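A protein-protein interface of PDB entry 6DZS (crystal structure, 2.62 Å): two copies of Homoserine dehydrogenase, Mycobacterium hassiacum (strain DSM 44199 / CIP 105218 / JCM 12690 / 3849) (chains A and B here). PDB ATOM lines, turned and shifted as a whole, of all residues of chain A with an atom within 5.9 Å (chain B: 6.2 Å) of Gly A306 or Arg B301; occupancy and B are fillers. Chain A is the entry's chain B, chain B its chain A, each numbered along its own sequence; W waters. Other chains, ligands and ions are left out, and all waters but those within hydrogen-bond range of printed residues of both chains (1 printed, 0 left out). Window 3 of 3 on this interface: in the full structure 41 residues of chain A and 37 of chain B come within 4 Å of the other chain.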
ATOM      1  N   ALA A 136      -5.004 -27.012  20.251  1.00  0.00           N
ATOM      2  CA  ALA A 136      -3.852 -26.120  20.215  1.00  0.00           C
ATOM      3  C   ALA A 136      -2.530 -26.872  20.269  1.00  0.00           C
ATOM      4  O   ALA A 136      -1.519 -26.316  20.706  1.00  0.00           O
ATOM      5  CB  ALA A 136      -3.909 -25.105  21.359  1.00  0.00           C
ATOM      6  N   ILE A 139       0.246 -26.056  22.782  1.00  0.00           N
ATOM      7  CA  ILE A 139      -0.127 -24.910  23.605  1.00  0.00           C
ATOM      8  C   ILE A 139      -1.067 -25.379  24.709  1.00  0.00           C
ATOM      9  O   ILE A 139      -2.177 -25.845  24.413  1.00  0.00           O
ATOM     10  CB  ILE A 139      -0.791 -23.807  22.766  1.00  0.00           C
ATOM     11  CG1 ILE A 139       0.055 -23.480  21.535  1.00  0.00           C
ATOM     12  CG2 ILE A 139      -1.007 -22.561  23.622  1.00  0.00           C
ATOM     13  CD1 ILE A 139      -0.599 -22.485  20.589  1.00  0.00           C
ATOM     14  N   VAL A 285       1.481 -14.296  13.751  1.00  0.00           N
ATOM     15  CA  VAL A 285       1.477 -15.738  13.980  1.00  0.00           C
ATOM     16  C   VAL A 285       1.517 -16.410  12.611  1.00  0.00           C
ATOM     17  O   VAL A 285       0.506 -16.477  11.911  1.00  0.00           O
ATOM     18  CB  VAL A 285       0.254 -16.176  14.787  1.00  0.00           C
ATOM     19  CG1 VAL A 285       0.312 -17.664  15.083  1.00  0.00           C
ATOM     20  CG2 VAL A 285       0.154 -15.380  16.073  1.00  0.00           C
ATOM     21  N   ALA A 288       3.224 -22.921  10.854  1.00  0.00           N
ATOM     22  CA  ALA A 288       2.352 -23.885  11.507  1.00  0.00           C
ATOM     23  C   ALA A 288       2.081 -23.538  12.962  1.00  0.00           C
ATOM     24  O   ALA A 288       1.625 -24.401  13.721  1.00  0.00           O
ATOM     25  CB  ALA A 288       2.955 -25.287  11.415  1.00  0.00           C
ATOM     26  N   PHE A 289       2.352 -22.305  13.373  1.00  0.00           N
ATOM     27  CA  PHE A 289       2.117 -21.931  14.757  1.00  0.00           C
ATOM     28  C   PHE A 289       0.653 -21.567  14.963  1.00  0.00           C
ATOM     29  O   PHE A 289      -0.076 -21.250  14.021  1.00  0.00           O
ATOM     30  CB  PHE A 289       3.005 -20.755  15.163  1.00  0.00           C
ATOM     31  CG  PHE A 289       4.463 -21.095  15.237  1.00  0.00           C
ATOM     32  CD1 PHE A 289       5.246 -21.074  14.103  1.00  0.00           C
ATOM     33  CD2 PHE A 289       5.049 -21.434  16.445  1.00  0.00           C
ATOM     34  CE1 PHE A 289       6.589 -21.388  14.166  1.00  0.00           C
ATOM     35  CE2 PHE A 289       6.395 -21.748  16.512  1.00  0.00           C
ATOM     36  CZ  PHE A 289       7.163 -21.723  15.369  1.00  0.00           C
ATOM     37  N   ASN A 290       0.228 -21.626  16.219  1.00  0.00           N
ATOM     38  CA  ASN A 290      -1.112 -21.231  16.619  1.00  0.00           C
ATOM     39  C   ASN A 290      -1.018 -20.173  17.713  1.00  0.00           C
ATOM     40  O   ASN A 290       0.045 -19.934  18.295  1.00  0.00           O
ATOM     41  CB  ASN A 290      -1.927 -22.435  17.108  1.00  0.00           C
ATOM     42  CG  ASN A 290      -2.383 -23.360  15.973  1.00  0.00           C
ATOM     43  OD1 ASN A 290      -2.980 -24.407  16.230  1.00  0.00           O
ATOM     44  ND2 ASN A 290      -2.103 -22.983  14.725  1.00  0.00           N
ATOM     45  N   ALA A 291      -2.149 -19.526  17.980  1.00  0.00           N
ATOM     46  CA  ALA A 291      -2.216 -18.519  19.030  1.00  0.00           C
ATOM     47  C   ALA A 291      -3.660 -18.367  19.477  1.00  0.00           C
ATOM     48  O   ALA A 291      -4.559 -18.239  18.642  1.00  0.00           O
ATOM     49  CB  ALA A 291      -1.662 -17.177  18.549  1.00  0.00           C
ATOM     50  N   PHE A 304      -1.784 -17.096  24.328  1.00  0.00           N
ATOM     51  CA  PHE A 304      -0.976 -18.307  24.377  1.00  0.00           C
ATOM     52  C   PHE A 304      -0.479 -18.612  22.970  1.00  0.00           C
ATOM     53  O   PHE A 304      -1.286 -18.721  22.042  1.00  0.00           O
ATOM     54  CB  PHE A 304      -1.797 -19.477  24.926  1.00  0.00           C
ATOM     55  CG  PHE A 304      -2.434 -19.201  26.261  1.00  0.00           C
ATOM     56  CD1 PHE A 304      -3.647 -18.533  26.343  1.00  0.00           C
ATOM     57  CD2 PHE A 304      -1.826 -19.619  27.433  1.00  0.00           C
ATOM     58  CE1 PHE A 304      -4.236 -18.278  27.573  1.00  0.00           C
ATOM     59  CE2 PHE A 304      -2.414 -19.369  28.664  1.00  0.00           C
ATOM     60  CZ  PHE A 304      -3.619 -18.698  28.731  1.00  0.00           C
ATOM     61  N   TYR A 305       0.842 -18.750  22.812  1.00  0.00           N
ATOM     62  CA  TYR A 305       1.479 -18.929  21.512  1.00  0.00           C
ATOM     63  C   TYR A 305       2.342 -20.185  21.520  1.00  0.00           C
ATOM     64  O   TYR A 305       3.022 -20.480  22.507  1.00  0.00           O
ATOM     65  CB  TYR A 305       2.329 -17.690  21.151  1.00  0.00           C
ATOM     66  CG  TYR A 305       3.204 -17.814  19.913  1.00  0.00           C
ATOM     67  CD1 TYR A 305       2.678 -17.637  18.634  1.00  0.00           C
ATOM     68  CD2 TYR A 305       4.568 -18.075  20.025  1.00  0.00           C
ATOM     69  CE1 TYR A 305       3.485 -17.737  17.504  1.00  0.00           C
ATOM     70  CE2 TYR A 305       5.379 -18.176  18.903  1.00  0.00           C
ATOM     71  CZ  TYR A 305       4.836 -18.004  17.647  1.00  0.00           C
ATOM     72  OH  TYR A 305       5.657 -18.107  16.544  1.00  0.00           O
ATOM     73  N   GLY A 306       2.303 -20.923  20.415  1.00  0.00           N
ATOM     74  CA  GLY A 306       3.122 -22.108  20.270  1.00  0.00           C
ATOM     75  C   GLY A 306       2.765 -22.857  19.000  1.00  0.00           C
ATOM     76  O   GLY A 306       2.006 -22.371  18.161  1.00  0.00           O
ATOM     77  N   GLN A 307       3.327 -24.056  18.882  1.00  0.00           N
ATOM     78  CA  GLN A 307       3.031 -24.923  17.747  1.00  0.00           C
ATOM     79  C   GLN A 307       1.706 -25.644  17.959  1.00  0.00           C
ATOM     80  O   GLN A 307       1.489 -26.275  18.998  1.00  0.00           O
ATOM     81  CB  GLN A 307       4.151 -25.935  17.545  1.00  0.00           C
ATOM     82  CG  GLN A 307       5.294 -25.395  16.732  1.00  0.00           C
ATOM     83  CD  GLN A 307       6.552 -26.204  16.913  1.00  0.00           C
ATOM     84  OE1 GLN A 307       7.571 -25.692  17.379  1.00  0.00           O
ATOM     85  NE2 GLN A 307       6.493 -27.479  16.544  1.00  0.00           N
ATOM     86  N   GLY A 308       0.827 -25.561  16.963  1.00  0.00           N
ATOM     87  CA  GLY A 308      -0.494 -26.141  17.081  1.00  0.00           C
ATOM     88  C   GLY A 308      -0.669 -27.424  16.295  1.00  0.00           C
ATOM     89  O   GLY A 308      -1.703 -28.090  16.393  1.00  0.00           O
ATOM     90  N   ARG B 156      14.586 -24.129  29.038  1.00  0.00           N
ATOM     91  CA  ARG B 156      14.799 -22.696  29.160  1.00  0.00           C
ATOM     92  C   ARG B 156      13.468 -22.050  29.503  1.00  0.00           C
ATOM     93  O   ARG B 156      12.457 -22.321  28.851  1.00  0.00           O
ATOM     94  CB  ARG B 156      15.360 -22.115  27.859  1.00  0.00           C
ATOM     95  CG  ARG B 156      15.877 -20.699  27.965  1.00  0.00           C
ATOM     96  CD  ARG B 156      16.472 -20.241  26.637  1.00  0.00           C
ATOM     97  NE  ARG B 156      17.410 -19.135  26.820  1.00  0.00           N
ATOM     98  CZ  ARG B 156      17.206 -17.877  26.427  1.00  0.00           C
ATOM     99  NH1 ARG B 156      16.088 -17.522  25.793  1.00  0.00           N
ATOM    100  NH2 ARG B 156      18.141 -16.964  26.661  1.00  0.00           N
ATOM    101  N   HIS B 280      12.929 -11.123  17.830  1.00  0.00           N
ATOM    102  CA  HIS B 280      12.546 -12.002  18.921  1.00  0.00           C
ATOM    103  C   HIS B 280      11.151 -11.636  19.425  1.00  0.00           C
ATOM    104  O   HIS B 280      10.757 -10.468  19.390  1.00  0.00           O
ATOM    105  CB  HIS B 280      13.559 -11.899  20.058  1.00  0.00           C
ATOM    106  CG  HIS B 280      13.507 -13.041  21.024  1.00  0.00           C
ATOM    107  ND1 HIS B 280      12.664 -13.056  22.114  1.00  0.00           N
ATOM    108  CD2 HIS B 280      14.199 -14.204  21.067  1.00  0.00           C
ATOM    109  CE1 HIS B 280      12.835 -14.182  22.784  1.00  0.00           C
ATOM    110  NE2 HIS B 280      13.760 -14.895  22.170  1.00  0.00           N
ATOM    111  N   PRO B 281      10.375 -12.620  19.888  1.00  0.00           N
ATOM    112  CA  PRO B 281       9.030 -12.289  20.394  1.00  0.00           C
ATOM    113  C   PRO B 281       9.041 -11.324  21.569  1.00  0.00           C
ATOM    114  O   PRO B 281       8.160 -10.460  21.665  1.00  0.00           O
ATOM    115  CB  PRO B 281       8.459 -13.658  20.798  1.00  0.00           C
ATOM    116  CG  PRO B 281       9.245 -14.654  20.022  1.00  0.00           C
ATOM    117  CD  PRO B 281      10.618 -14.074  19.867  1.00  0.00           C
ATOM    118  N   VAL B 293       8.643 -17.033  28.033  1.00  0.00           N
ATOM    119  CA  VAL B 293       8.990 -17.984  26.979  1.00  0.00           C
ATOM    120  C   VAL B 293       9.496 -19.268  27.621  1.00  0.00           C
ATOM    121  O   VAL B 293      10.361 -19.234  28.505  1.00  0.00           O
ATOM    122  CB  VAL B 293      10.043 -17.395  26.024  1.00  0.00           C
ATOM    123  CG1 VAL B 293      10.445 -18.416  24.978  1.00  0.00           C
ATOM    124  CG2 VAL B 293       9.504 -16.137  25.361  1.00  0.00           C
ATOM    125  N   VAL B 294       8.967 -20.402  27.173  1.00  0.00           N
ATOM    126  CA  VAL B 294       9.338 -21.713  27.699  1.00  0.00           C
ATOM    127  C   VAL B 294       9.793 -22.579  26.532  1.00  0.00           C
ATOM    128  O   VAL B 294       9.042 -22.779  25.570  1.00  0.00           O
ATOM    129  CB  VAL B 294       8.172 -22.372  28.456  1.00  0.00           C
ATOM    130  CG1 VAL B 294       8.545 -23.767  28.935  1.00  0.00           C
ATOM    131  CG2 VAL B 294       7.762 -21.502  29.636  1.00  0.00           C
ATOM    132  N   GLU B 295      11.026 -23.077  26.612  1.00  0.00           N
ATOM    133  CA  GLU B 295      11.566 -24.015  25.633  1.00  0.00           C
ATOM    134  C   GLU B 295      11.504 -25.420  26.222  1.00  0.00           C
ATOM    135  O   GLU B 295      12.091 -25.683  27.277  1.00  0.00           O
ATOM    136  CB  GLU B 295      13.009 -23.673  25.263  1.00  0.00           C
ATOM    137  CG  GLU B 295      13.211 -22.311  24.623  1.00  0.00           C
ATOM    138  CD  GLU B 295      12.752 -22.257  23.182  1.00  0.00           C
ATOM    139  OE1 GLU B 295      12.439 -23.324  22.608  1.00  0.00           O
ATOM    140  OE2 GLU B 295      12.706 -21.139  22.621  1.00  0.00           O
ATOM    141  N   ALA B 296      10.796 -26.314  25.547  1.00  0.00           N
ATOM    142  CA  ALA B 296      10.783 -27.724  25.906  1.00  0.00           C
ATOM    143  C   ALA B 296      11.169 -28.541  24.683  1.00  0.00           C
ATOM    144  O   ALA B 296      11.144 -28.052  23.550  1.00  0.00           O
ATOM    145  CB  ALA B 296       9.417 -28.172  26.433  1.00  0.00           C
ATOM    146  N   ALA B 299       7.686 -29.979  22.873  1.00  0.00           N
ATOM    147  CA  ALA B 299       6.721 -28.935  22.567  1.00  0.00           C
ATOM    148  C   ALA B 299       7.332 -27.768  21.815  1.00  0.00           C
ATOM    149  O   ALA B 299       6.600 -27.029  21.148  1.00  0.00           O
ATOM    150  CB  ALA B 299       6.080 -28.416  23.859  1.00  0.00           C
ATOM    151  N   GLY B 300       8.642 -27.577  21.913  1.00  0.00           N
ATOM    152  CA  GLY B 300       9.278 -26.456  21.263  1.00  0.00           C
ATOM    153  C   GLY B 300       9.119 -25.190  22.071  1.00  0.00           C
ATOM    154  O   GLY B 300       9.246 -25.211  23.299  1.00  0.00           O
ATOM    155  N   ARG B 301       8.823 -24.087  21.394  1.00  0.00           N
ATOM    156  CA  ARG B 301       8.756 -22.777  22.022  1.00  0.00           C
ATOM    157  C   ARG B 301       7.307 -22.396  22.298  1.00  0.00           C
ATOM    158  O   ARG B 301       6.471 -22.409  21.391  1.00  0.00           O
ATOM    159  CB  ARG B 301       9.425 -21.725  21.137  1.00  0.00           C
ATOM    160  CG  ARG B 301       9.241 -20.299  21.622  1.00  0.00           C
ATOM    161  CD  ARG B 301       9.820 -19.313  20.633  1.00  0.00           C
ATOM    162  NE  ARG B 301      11.253 -19.145  20.821  1.00  0.00           N
ATOM    163  CZ  ARG B 301      11.995 -18.290  20.130  1.00  0.00           C
ATOM    164  NH1 ARG B 301      11.434 -17.530  19.197  1.00  0.00           N
ATOM    165  NH2 ARG B 301      13.296 -18.196  20.372  1.00  0.00           N
ATOM    166  N   LEU B 302       7.023 -22.059  23.551  1.00  0.00           N
ATOM    167  CA  LEU B 302       5.730 -21.544  23.973  1.00  0.00           C
ATOM    168  C   LEU B 302       5.918 -20.146  24.543  1.00  0.00           C
ATOM    169  O   LEU B 302       6.961 -19.840  25.130  1.00  0.00           O
ATOM    170  CB  LEU B 302       5.093 -22.448  25.033  1.00  0.00           C
ATOM    171  CG  LEU B 302       4.832 -23.906  24.669  1.00  0.00           C
ATOM    172  CD1 LEU B 302       4.550 -24.731  25.909  1.00  0.00           C
ATOM    173  CD2 LEU B 302       3.664 -23.999  23.718  1.00  0.00           C
ATOM    174  N   MET B 303       4.911 -19.291  24.370  1.00  0.00           N
ATOM    175  CA  MET B 303       4.948 -17.959  24.965  1.00  0.00           C
ATOM    176  C   MET B 303       3.606 -17.643  25.607  1.00  0.00           C
ATOM    177  O   MET B 303       2.555 -17.829  24.987  1.00  0.00           O
ATOM    178  CB  MET B 303       5.300 -16.874  23.936  1.00  0.00           C
ATOM    179  CG  MET B 303       5.759 -15.567  24.606  1.00  0.00           C
ATOM    180  SD  MET B 303       6.012 -14.149  23.515  1.00  0.00           S
ATOM    181  CE  MET B 303       4.333 -13.546  23.290  1.00  0.00           C
HETATM  182  O   HOH W   1       9.204 -24.046  18.270  1.00  0.00           O
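Of the printed residues of chain B, Gly A306 touches Arg B301 (3.5 Å) and Leu B302 (3.97 Å).
Of the printed residues of chain A, Met B303 touches Phe A304 (3.6 Å) and Tyr A305 (2.9 Å).
Printed residues of chain B within 4 Å of Phe A304: Met B303 (3.6 Å).
Printed residues of chain B within 4 Å of Ile A139: Leu B302 (3.9 Å).
Of the printed residues of chain B, Tyr A305 touches Leu B302 and Met B303.
Of the printed residues of chain A, Leu B302 touches Ile A139 (3.9 Å), Tyr A305 (3.3 Å) and Gly A306 (3.97 Å).
Ala B296 touches none of the printed residues of chain A.
The nearest printed residue of chain A that does not touch Leu B302 is Gln A307 (4.8 Å).
Leu B302 touches Ile A139.
Met B303 touches Phe A304.
Tyr A305 touches Leu B302 (O to CA, 3.3 Å).
Gly A306 touches Arg B301.
Gly A306 touches Leu B302 (CA to CD2, 3.97 Å).
The backbone NH (N) of Val B294 sits at hydrogen-bond distance from the backbone carbonyl oxygen (O) of Leu B302 (2.9 Å).
OE2 of Glu B295 lies within salt-bridge range of NE of Arg B301.
The backbone NH (N) of Asn A290 is in hydrogen-bond range of the backbone carbonyl oxygen (O) of Gly A306, at 2.7 Å.
Water W1 bridges OE1 of Gln A307 and N of Arg B301.
Hydrophobic or aromatic side chains of chain B that line the printed part of chain A: Leu B302.
Hydrophobic or aromatic side chains of chain A within 4 Å of the printed part of chain B: Tyr A305.
Among the printed residues, 6 pairs touch across the chains.
Among the printed residues, no Asp or Glu carboxylate lies within 4 Å of a Lys or Arg side-chain nitrogen of the other chain.
No position is printed for both chains.
The backbone NH of Met B303 is in hydrogen-bond range of the backbone carbonyl oxygen of Tyr A305 (2.9 Å).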
